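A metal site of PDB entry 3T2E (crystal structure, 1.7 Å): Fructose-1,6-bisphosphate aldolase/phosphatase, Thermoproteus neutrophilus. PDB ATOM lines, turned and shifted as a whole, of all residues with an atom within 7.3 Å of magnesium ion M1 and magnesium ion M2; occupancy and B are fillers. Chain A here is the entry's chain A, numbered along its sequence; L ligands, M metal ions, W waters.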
ATOM      1  N   LYS A   9       8.971  -0.479  -4.812  1.00  0.00           N
ATOM      2  CA  LYS A   9      10.322  -0.047  -5.287  1.00  0.00           C
ATOM      3  C   LYS A   9      10.185   1.132  -6.192  1.00  0.00           C
ATOM      4  O   LYS A   9       9.181   1.184  -6.938  1.00  0.00           O
ATOM      5  CB  LYS A   9      10.938  -1.264  -5.996  1.00  0.00           C
ATOM      6  CG  LYS A   9      12.315  -0.976  -6.722  1.00  0.00           C
ATOM      7  CD  LYS A   9      12.074  -1.103  -8.243  1.00  0.00           C
ATOM      8  CE  LYS A   9      11.981   0.140  -8.918  1.00  0.00           C
ATOM      9  NZ  LYS A   9      11.943   0.118 -10.467  1.00  0.00           N
ATOM     10  N   ALA A  10      11.106   2.091  -6.141  1.00  0.00           N
ATOM     11  CA  ALA A  10      11.075   3.216  -7.101  1.00  0.00           C
ATOM     12  C   ALA A  10      12.500   3.670  -7.267  1.00  0.00           C
ATOM     13  O   ALA A  10      13.319   3.603  -6.343  1.00  0.00           O
ATOM     14  CB  ALA A  10      10.265   4.400  -6.513  1.00  0.00           C
ATOM     15  N   ASP A  11      12.683   4.291  -8.413  1.00  0.00           N
ATOM     16  CA  ASP A  11      13.903   5.093  -8.616  1.00  0.00           C
ATOM     17  C   ASP A  11      13.503   6.580  -8.498  1.00  0.00           C
ATOM     18  O   ASP A  11      12.717   7.088  -9.391  1.00  0.00           O
ATOM     19  CB  ASP A  11      14.399   4.795 -10.019  1.00  0.00           C
ATOM     20  CG  ASP A  11      15.592   5.660 -10.481  1.00  0.00           C
ATOM     21  OD1 ASP A  11      15.982   6.705  -9.913  1.00  0.00           O
ATOM     22  OD2 ASP A  11      16.065   5.187 -11.553  1.00  0.00           O
ATOM     23  N   VAL A  12      13.975   7.277  -7.489  1.00  0.00           N
ATOM     24  CA  VAL A  12      13.638   8.672  -7.303  1.00  0.00           C
ATOM     25  C   VAL A  12      14.872   9.504  -7.404  1.00  0.00           C
ATOM     26  O   VAL A  12      14.903  10.597  -6.895  1.00  0.00           O
ATOM     27  CB  VAL A  12      12.841   8.972  -5.979  1.00  0.00           C
ATOM     28  CG1 VAL A  12      11.497   8.210  -6.048  1.00  0.00           C
ATOM     29  CG2 VAL A  12      13.598   8.482  -4.782  1.00  0.00           C
ATOM     30  N   GLY A  13      15.928   8.969  -8.026  1.00  0.00           N
ATOM     31  CA  GLY A  13      17.133   9.838  -8.214  1.00  0.00           C
ATOM     32  C   GLY A  13      18.392   8.993  -8.075  1.00  0.00           C
ATOM     33  O   GLY A  13      18.514   8.218  -7.196  1.00  0.00           O
ATOM     34  N   GLY A  14      19.302   9.215  -8.987  1.00  0.00           N
ATOM     35  CA  GLY A  14      20.587   8.460  -9.016  1.00  0.00           C
ATOM     36  C   GLY A  14      21.804   9.308  -8.703  1.00  0.00           C
ATOM     37  O   GLY A  14      21.791  10.564  -8.706  1.00  0.00           O
ATOM     38  N   GLY A  17      24.134  10.072 -12.129  1.00  0.00           N
ATOM     39  CA  GLY A  17      23.426   9.469 -13.286  1.00  0.00           C
ATOM     40  C   GLY A  17      22.475   8.395 -12.796  1.00  0.00           C
ATOM     41  O   GLY A  17      21.698   8.609 -11.819  1.00  0.00           O
ATOM     42  N   HIS A  18      22.541   7.225 -13.442  1.00  0.00           N
ATOM     43  CA  HIS A  18      21.696   6.097 -12.982  1.00  0.00           C
ATOM     44  C   HIS A  18      22.555   4.991 -12.326  1.00  0.00           C
ATOM     45  O   HIS A  18      22.168   3.821 -12.305  1.00  0.00           O
ATOM     46  CB  HIS A  18      20.962   5.528 -14.153  1.00  0.00           C
ATOM     47  CG  HIS A  18      20.007   6.516 -14.801  1.00  0.00           C
ATOM     48  ND1 HIS A  18      18.772   6.801 -14.259  1.00  0.00           N
ATOM     49  CD2 HIS A  18      20.087   7.225 -15.948  1.00  0.00           C
ATOM     50  CE1 HIS A  18      18.138   7.669 -15.014  1.00  0.00           C
ATOM     51  NE2 HIS A  18      18.907   7.949 -16.058  1.00  0.00           N
ATOM     52  N   ALA A  19      23.686   5.417 -11.791  1.00  0.00           N
ATOM     53  CA  ALA A  19      24.669   4.370 -11.375  1.00  0.00           C
ATOM     54  C   ALA A  19      24.409   3.792 -10.009  1.00  0.00           C
ATOM     55  O   ALA A  19      24.850   2.663  -9.698  1.00  0.00           O
ATOM     56  CB  ALA A  19      26.115   4.974 -11.369  1.00  0.00           C
ATOM     57  N   HIS A  20      23.789   4.608  -9.090  1.00  0.00           N
ATOM     58  CA  HIS A  20      23.680   4.140  -7.705  1.00  0.00           C
ATOM     59  C   HIS A  20      22.686   5.081  -7.013  1.00  0.00           C
ATOM     60  O   HIS A  20      22.131   5.941  -7.689  1.00  0.00           O
ATOM     61  CB  HIS A  20      25.036   4.301  -7.074  1.00  0.00           C
ATOM     62  CG  HIS A  20      25.341   3.349  -5.947  1.00  0.00           C
ATOM     63  ND1 HIS A  20      24.955   2.001  -5.875  1.00  0.00           N
ATOM     64  CD2 HIS A  20      26.160   3.543  -4.886  1.00  0.00           C
ATOM     65  CE1 HIS A  20      25.470   1.448  -4.765  1.00  0.00           C
ATOM     66  NE2 HIS A  20      26.217   2.365  -4.175  1.00  0.00           N
ATOM     67  N   VAL A  50      19.422  -1.685  -5.381  1.00  0.00           N
ATOM     68  CA  VAL A  50      20.407  -2.324  -6.344  1.00  0.00           C
ATOM     69  C   VAL A  50      20.479  -1.273  -7.453  1.00  0.00           C
ATOM     70  O   VAL A  50      19.426  -0.813  -8.032  1.00  0.00           O
ATOM     71  CB  VAL A  50      19.808  -3.639  -6.889  1.00  0.00           C
ATOM     72  CG1 VAL A  50      20.629  -4.185  -8.116  1.00  0.00           C
ATOM     73  CG2 VAL A  50      19.822  -4.771  -5.786  1.00  0.00           C
ATOM     74  N   GLY A  51      21.710  -0.781  -7.726  1.00  0.00           N
ATOM     75  CA  GLY A  51      21.742   0.307  -8.734  1.00  0.00           C
ATOM     76  C   GLY A  51      21.035   1.563  -8.184  1.00  0.00           C
ATOM     77  O   GLY A  51      21.174   1.948  -7.030  1.00  0.00           O
ATOM     78  N   ASP A  52      20.247   2.143  -9.062  1.00  0.00           N
ATOM     79  CA  ASP A  52      19.545   3.391  -8.697  1.00  0.00           C
ATOM     80  C   ASP A  52      18.109   3.103  -8.266  1.00  0.00           C
ATOM     81  O   ASP A  52      17.294   4.065  -8.173  1.00  0.00           O
ATOM     82  CB  ASP A  52      19.499   4.412  -9.880  1.00  0.00           C
ATOM     83  CG  ASP A  52      18.831   3.815 -11.128  1.00  0.00           C
ATOM     84  OD1 ASP A  52      18.357   2.632 -11.186  1.00  0.00           O
ATOM     85  OD2 ASP A  52      18.712   4.545 -12.193  1.00  0.00           O
ATOM     86  N   ASP A  53      17.799   1.858  -7.924  1.00  0.00           N
ATOM     87  CA  ASP A  53      16.418   1.516  -7.485  1.00  0.00           C
ATOM     88  C   ASP A  53      16.379   1.225  -6.019  1.00  0.00           C
ATOM     89  O   ASP A  53      17.086   0.320  -5.525  1.00  0.00           O
ATOM     90  CB  ASP A  53      15.907   0.301  -8.255  1.00  0.00           C
ATOM     91  CG  ASP A  53      15.622   0.740  -9.716  1.00  0.00           C
ATOM     92  OD1 ASP A  53      14.618   1.386 -10.020  1.00  0.00           O
ATOM     93  OD2 ASP A  53      16.480   0.432 -10.454  1.00  0.00           O
ATOM     94  N   ILE A  54      15.460   1.897  -5.290  1.00  0.00           N
ATOM     95  CA  ILE A  54      15.309   1.649  -3.846  1.00  0.00           C
ATOM     96  C   ILE A  54      14.067   0.760  -3.617  1.00  0.00           C
ATOM     97  O   ILE A  54      13.011   1.127  -4.055  1.00  0.00           O
ATOM     98  CB  ILE A  54      15.095   2.960  -3.100  1.00  0.00           C
ATOM     99  CG1 ILE A  54      16.393   3.798  -3.264  1.00  0.00           C
ATOM    100  CG2 ILE A  54      14.730   2.712  -1.587  1.00  0.00           C
ATOM    101  CD1 ILE A  54      16.221   5.260  -2.698  1.00  0.00           C
ATOM    102  N   TYR A  91      20.178  12.708 -10.302  1.00  0.00           N
ATOM    103  CA  TYR A  91      19.776  12.562 -11.650  1.00  0.00           C
ATOM    104  C   TYR A  91      18.510  11.718 -11.761  1.00  0.00           C
ATOM    105  O   TYR A  91      18.386  10.623 -11.228  1.00  0.00           O
ATOM    106  CB  TYR A  91      20.977  11.885 -12.504  1.00  0.00           C
ATOM    107  CG  TYR A  91      20.702  12.090 -13.962  1.00  0.00           C
ATOM    108  CD1 TYR A  91      20.924  13.331 -14.567  1.00  0.00           C
ATOM    109  CD2 TYR A  91      20.130  11.058 -14.747  1.00  0.00           C
ATOM    110  CE1 TYR A  91      20.567  13.594 -15.885  1.00  0.00           C
ATOM    111  CE2 TYR A  91      19.745  11.289 -16.110  1.00  0.00           C
ATOM    112  CZ  TYR A  91      19.995  12.584 -16.649  1.00  0.00           C
ATOM    113  OH  TYR A  91      19.632  12.867 -17.933  1.00  0.00           O
ATOM    114  N   GLY A  92      17.524  12.233 -12.528  1.00  0.00           N
ATOM    115  CA  GLY A  92      16.182  11.602 -12.534  1.00  0.00           C
ATOM    116  C   GLY A  92      15.449  11.825 -11.187  1.00  0.00           C
ATOM    117  O   GLY A  92      14.670  10.992 -10.743  1.00  0.00           O
ATOM    118  N   GLN A  95      12.031  10.646 -10.635  1.00  0.00           N
ATOM    119  CA  GLN A  95      11.848   9.863 -11.920  1.00  0.00           C
ATOM    120  C   GLN A  95      10.498   9.058 -11.904  1.00  0.00           C
ATOM    121  O   GLN A  95       9.583   9.289 -12.720  1.00  0.00           O
ATOM    122  CB  GLN A  95      13.137   8.944 -12.193  1.00  0.00           C
ATOM    123  CG  GLN A  95      13.201   8.047 -13.458  1.00  0.00           C
ATOM    124  CD  GLN A  95      14.641   7.709 -14.014  1.00  0.00           C
ATOM    125  OE1 GLN A  95      15.674   7.478 -13.283  1.00  0.00           O
ATOM    126  NE2 GLN A  95      14.695   7.670 -15.358  1.00  0.00           N
ATOM    127  N   ASP A  96      10.360   8.151 -10.942  1.00  0.00           N
ATOM    128  CA  ASP A  96       9.200   7.241 -10.982  1.00  0.00           C
ATOM    129  C   ASP A  96       7.909   7.766 -10.384  1.00  0.00           C
ATOM    130  O   ASP A  96       6.929   7.015 -10.347  1.00  0.00           O
ATOM    131  CB  ASP A  96       9.545   5.887 -10.324  1.00  0.00           C
ATOM    132  CG  ASP A  96      10.457   5.076 -11.135  1.00  0.00           C
ATOM    133  OD1 ASP A  96      10.743   5.429 -12.335  1.00  0.00           O
ATOM    134  OD2 ASP A  96      10.991   4.088 -10.586  1.00  0.00           O
ATOM    135  N   ALA A 131      16.305  -6.244  -9.251  1.00  0.00           N
ATOM    136  CA  ALA A 131      17.253  -6.155 -10.407  1.00  0.00           C
ATOM    137  C   ALA A 131      17.266  -4.745 -10.928  1.00  0.00           C
ATOM    138  O   ALA A 131      16.259  -4.059 -10.830  1.00  0.00           O
ATOM    139  CB  ALA A 131      16.844  -7.138 -11.503  1.00  0.00           C
ATOM    140  N   ASP A 132      18.410  -4.183 -11.342  1.00  0.00           N
ATOM    141  CA  ASP A 132      18.403  -2.877 -11.969  1.00  0.00           C
ATOM    142  C   ASP A 132      18.824  -3.068 -13.451  1.00  0.00           C
ATOM    143  O   ASP A 132      19.505  -4.053 -13.851  1.00  0.00           O
ATOM    144  CB  ASP A 132      19.477  -1.997 -11.261  1.00  0.00           C
ATOM    145  CG  ASP A 132      19.439  -0.520 -11.737  1.00  0.00           C
ATOM    146  OD1 ASP A 132      18.396  -0.116 -12.338  1.00  0.00           O
ATOM    147  OD2 ASP A 132      20.451   0.151 -11.541  1.00  0.00           O
ATOM    148  N   LYS A 133      18.373  -2.101 -14.245  1.00  0.00           N
ATOM    149  CA  LYS A 133      18.670  -2.025 -15.676  1.00  0.00           C
ATOM    150  C   LYS A 133      18.108  -3.176 -16.458  1.00  0.00           C
ATOM    151  O   LYS A 133      18.715  -3.728 -17.399  1.00  0.00           O
ATOM    152  CB  LYS A 133      20.236  -1.911 -15.917  1.00  0.00           C
ATOM    153  CG  LYS A 133      20.903  -0.758 -15.082  1.00  0.00           C
ATOM    154  CD  LYS A 133      20.448   0.594 -15.674  1.00  0.00           C
ATOM    155  CE  LYS A 133      21.103   1.754 -14.941  1.00  0.00           C
ATOM    156  NZ  LYS A 133      20.442   2.073 -13.593  1.00  0.00           N
ATOM    157  N   THR A 134      16.861  -3.568 -16.107  1.00  0.00           N
ATOM    158  CA  THR A 134      16.196  -4.570 -16.916  1.00  0.00           C
ATOM    159  C   THR A 134      14.675  -4.481 -16.674  1.00  0.00           C
ATOM    160  O   THR A 134      14.247  -3.565 -16.007  1.00  0.00           O
ATOM    161  CB  THR A 134      16.809  -5.994 -16.631  1.00  0.00           C
ATOM    162  OG1 THR A 134      16.235  -6.918 -17.555  1.00  0.00           O
ATOM    163  CG2 THR A 134      16.527  -6.479 -15.208  1.00  0.00           C
ATOM    164  N   ASP A 233       9.677  -0.941 -15.969  1.00  0.00           N
ATOM    165  CA  ASP A 233      10.447  -0.465 -14.913  1.00  0.00           C
ATOM    166  C   ASP A 233      11.187  -1.660 -14.224  1.00  0.00           C
ATOM    167  O   ASP A 233      10.634  -2.824 -14.188  1.00  0.00           O
ATOM    168  CB  ASP A 233       9.532   0.280 -13.908  1.00  0.00           C
ATOM    169  CG  ASP A 233       8.555   1.266 -14.642  1.00  0.00           C
ATOM    170  OD1 ASP A 233       9.039   2.401 -14.815  1.00  0.00           O
ATOM    171  OD2 ASP A 233       7.389   0.820 -15.004  1.00  0.00           O
ATOM    172  N   ASP A 234      12.333  -1.345 -13.665  1.00  0.00           N
ATOM    173  CA  ASP A 234      13.264  -2.404 -13.108  1.00  0.00           C
ATOM    174  C   ASP A 234      12.478  -3.167 -12.008  1.00  0.00           C
ATOM    175  O   ASP A 234      11.798  -2.514 -11.154  1.00  0.00           O
ATOM    176  CB  ASP A 234      14.458  -1.732 -12.466  1.00  0.00           C
ATOM    177  CG  ASP A 234      15.279  -0.865 -13.445  1.00  0.00           C
ATOM    178  OD1 ASP A 234      15.320  -1.276 -14.610  1.00  0.00           O
ATOM    179  OD2 ASP A 234      15.786   0.217 -13.118  1.00  0.00           O
ATOM    180  N   MET A 293      25.982   0.432 -10.961  1.00  0.00           N
ATOM    181  CA  MET A 293      25.989   0.146 -12.423  1.00  0.00           C
ATOM    182  C   MET A 293      27.084   1.023 -13.028  1.00  0.00           C
ATOM    183  O   MET A 293      27.169   2.229 -12.734  1.00  0.00           O
ATOM    184  CB  MET A 293      24.624   0.530 -13.070  1.00  0.00           C
ATOM    185  CG  MET A 293      23.441  -0.100 -12.384  1.00  0.00           C
ATOM    186  SD  MET A 293      23.582  -1.965 -12.375  1.00  0.00           S
ATOM    187  CE  MET A 293      23.390  -2.210 -10.750  1.00  0.00           C
HETATM  188  C1  LIG L   1      18.342   2.961 -18.577  1.00  0.00           C
HETATM  189  C2  LIG L   1      18.697   4.096 -17.977  1.00  0.00           C
HETATM  190  C3  LIG L   1      19.972   4.757 -18.416  1.00  0.00           C
HETATM  191  C4  LIG L   1      19.644   6.050 -19.199  1.00  0.00           C
HETATM  192  C5  LIG L   1      20.890   6.720 -19.781  1.00  0.00           C
HETATM  193  C6  LIG L   1      20.675   7.982 -20.667  1.00  0.00           C
HETATM  194  O1  LIG L   1      17.151   2.477 -18.065  1.00  0.00           O
HETATM  195  O2  LIG L   1      17.942   4.683 -17.143  1.00  0.00           O
HETATM  196  O3  LIG L   1      20.734   3.768 -19.204  1.00  0.00           O
HETATM  197  O4  LIG L   1      18.730   5.763 -20.256  1.00  0.00           O
HETATM  198  O5  LIG L   1      21.810   6.971 -18.714  1.00  0.00           O
HETATM  199  O6  LIG L   1      19.890   8.843 -19.781  1.00  0.00           O
HETATM  200  P1  LIG L   1      19.692  10.341 -20.406  1.00  0.00           P
HETATM  201  O7  LIG L   1      18.692  10.961 -19.399  1.00  0.00           O
HETATM  202  O8  LIG L   1      19.050  10.176 -21.750  1.00  0.00           O
HETATM  203  O9  LIG L   1      20.993  11.069 -20.407  1.00  0.00           O
HETATM  204 MG    MG M   1      17.040   1.466 -12.272  1.00  0.00          MG
HETATM  205 MG    MG M   2      17.506   6.008 -12.786  1.00  0.00          MG
HETATM  206  O   HOH W   1      16.543   4.875 -14.162  1.00  0.00           O
HETATM  207  O   HOH W   2      15.512   2.640 -12.235  1.00  0.00           O
HETATM  208  O   HOH W   3      18.042   7.274 -11.534  1.00  0.00           O
HETATM  209  O   HOH W   4      17.648   2.379 -14.044  1.00  0.00           O
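Lys 133 touches magnesium ion M1. Within 4 Å of magnesium ion M1: Asp 11, Asp 52, Asp 53, Asp 132, Lys 133 and Asp 234.
Magnesium ion M2 is bound by water W3 (1.9 Å), the side-chain carboxylate (OD2) of Asp 52 (2.0 Å), water W1 (2.0 Å), the side-chain carboxylate (OD2) of Asp 11 (2.1 Å), a ring nitrogen (ND1) of His 18 (2.1 Å) and the side-chain amide oxygen (OE1) of Gln 95 (2.4 Å).
O7 of the ligand lies within hydrogen-bond range of OH of Tyr 91, at 2.6 Å.
Magnesium ion M1 is bound by water W2 (1.9 Å). OD2 of Asp 234 is bound to magnesium ion M1 (2.0 Å). Magnesium ion M1 is bound by OD1 of Asp 52, 2.1 Å away. Water W4 is bound to magnesium ion M1, 2.1 Å away. OD1 of Asp 132 is bound to magnesium ion M1 (2.1 Å). Magnesium ion M1 is bound by OD2 of Asp 53 (2.2 Å).
Within 4 Å of magnesium ion M2: Asp 11, His 18, Asp 52 and Gln 95.
The side-chain carboxylate (OD1) of Asp 234 sits at hydrogen-bond distance from the backbone NH (N) of Lys 133. O of Asp 234 sits at hydrogen-bond distance from NZ of Lys 9, at 2.7 Å. OD1 of Asp 234 sits at hydrogen-bond distance from N of Thr 134, 3.1 Å away. The side-chain carboxylate (OD1) of Asp 52 sits close to the side-chain amino group (NZ) of Lys 133 (3.2 Å). The side-chain carboxylate (OD1) of Asp 11 is in hydrogen-bond range of the backbone NH (N) of Gly 13 (2.9 Å). The side-chain carboxylate (OD2) of Asp 132 is in salt-bridge range of the side-chain amino group (NZ) of Lys 133 (2.8 Å). O of His 18 is in hydrogen-bond range of NZ of Lys 133 (2.8 Å). The side-chain carboxylate (OD1) of Asp 53 lies within salt-bridge range of the side-chain amino group (NZ) of Lys 9, at 3.0 Å.
Water W3 lies within hydrogen-bond range of OD1 of Asp 11 (2.7 Å), O of Tyr 91 (3.4 Å) and N of Gly 14 (3.4 Å).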
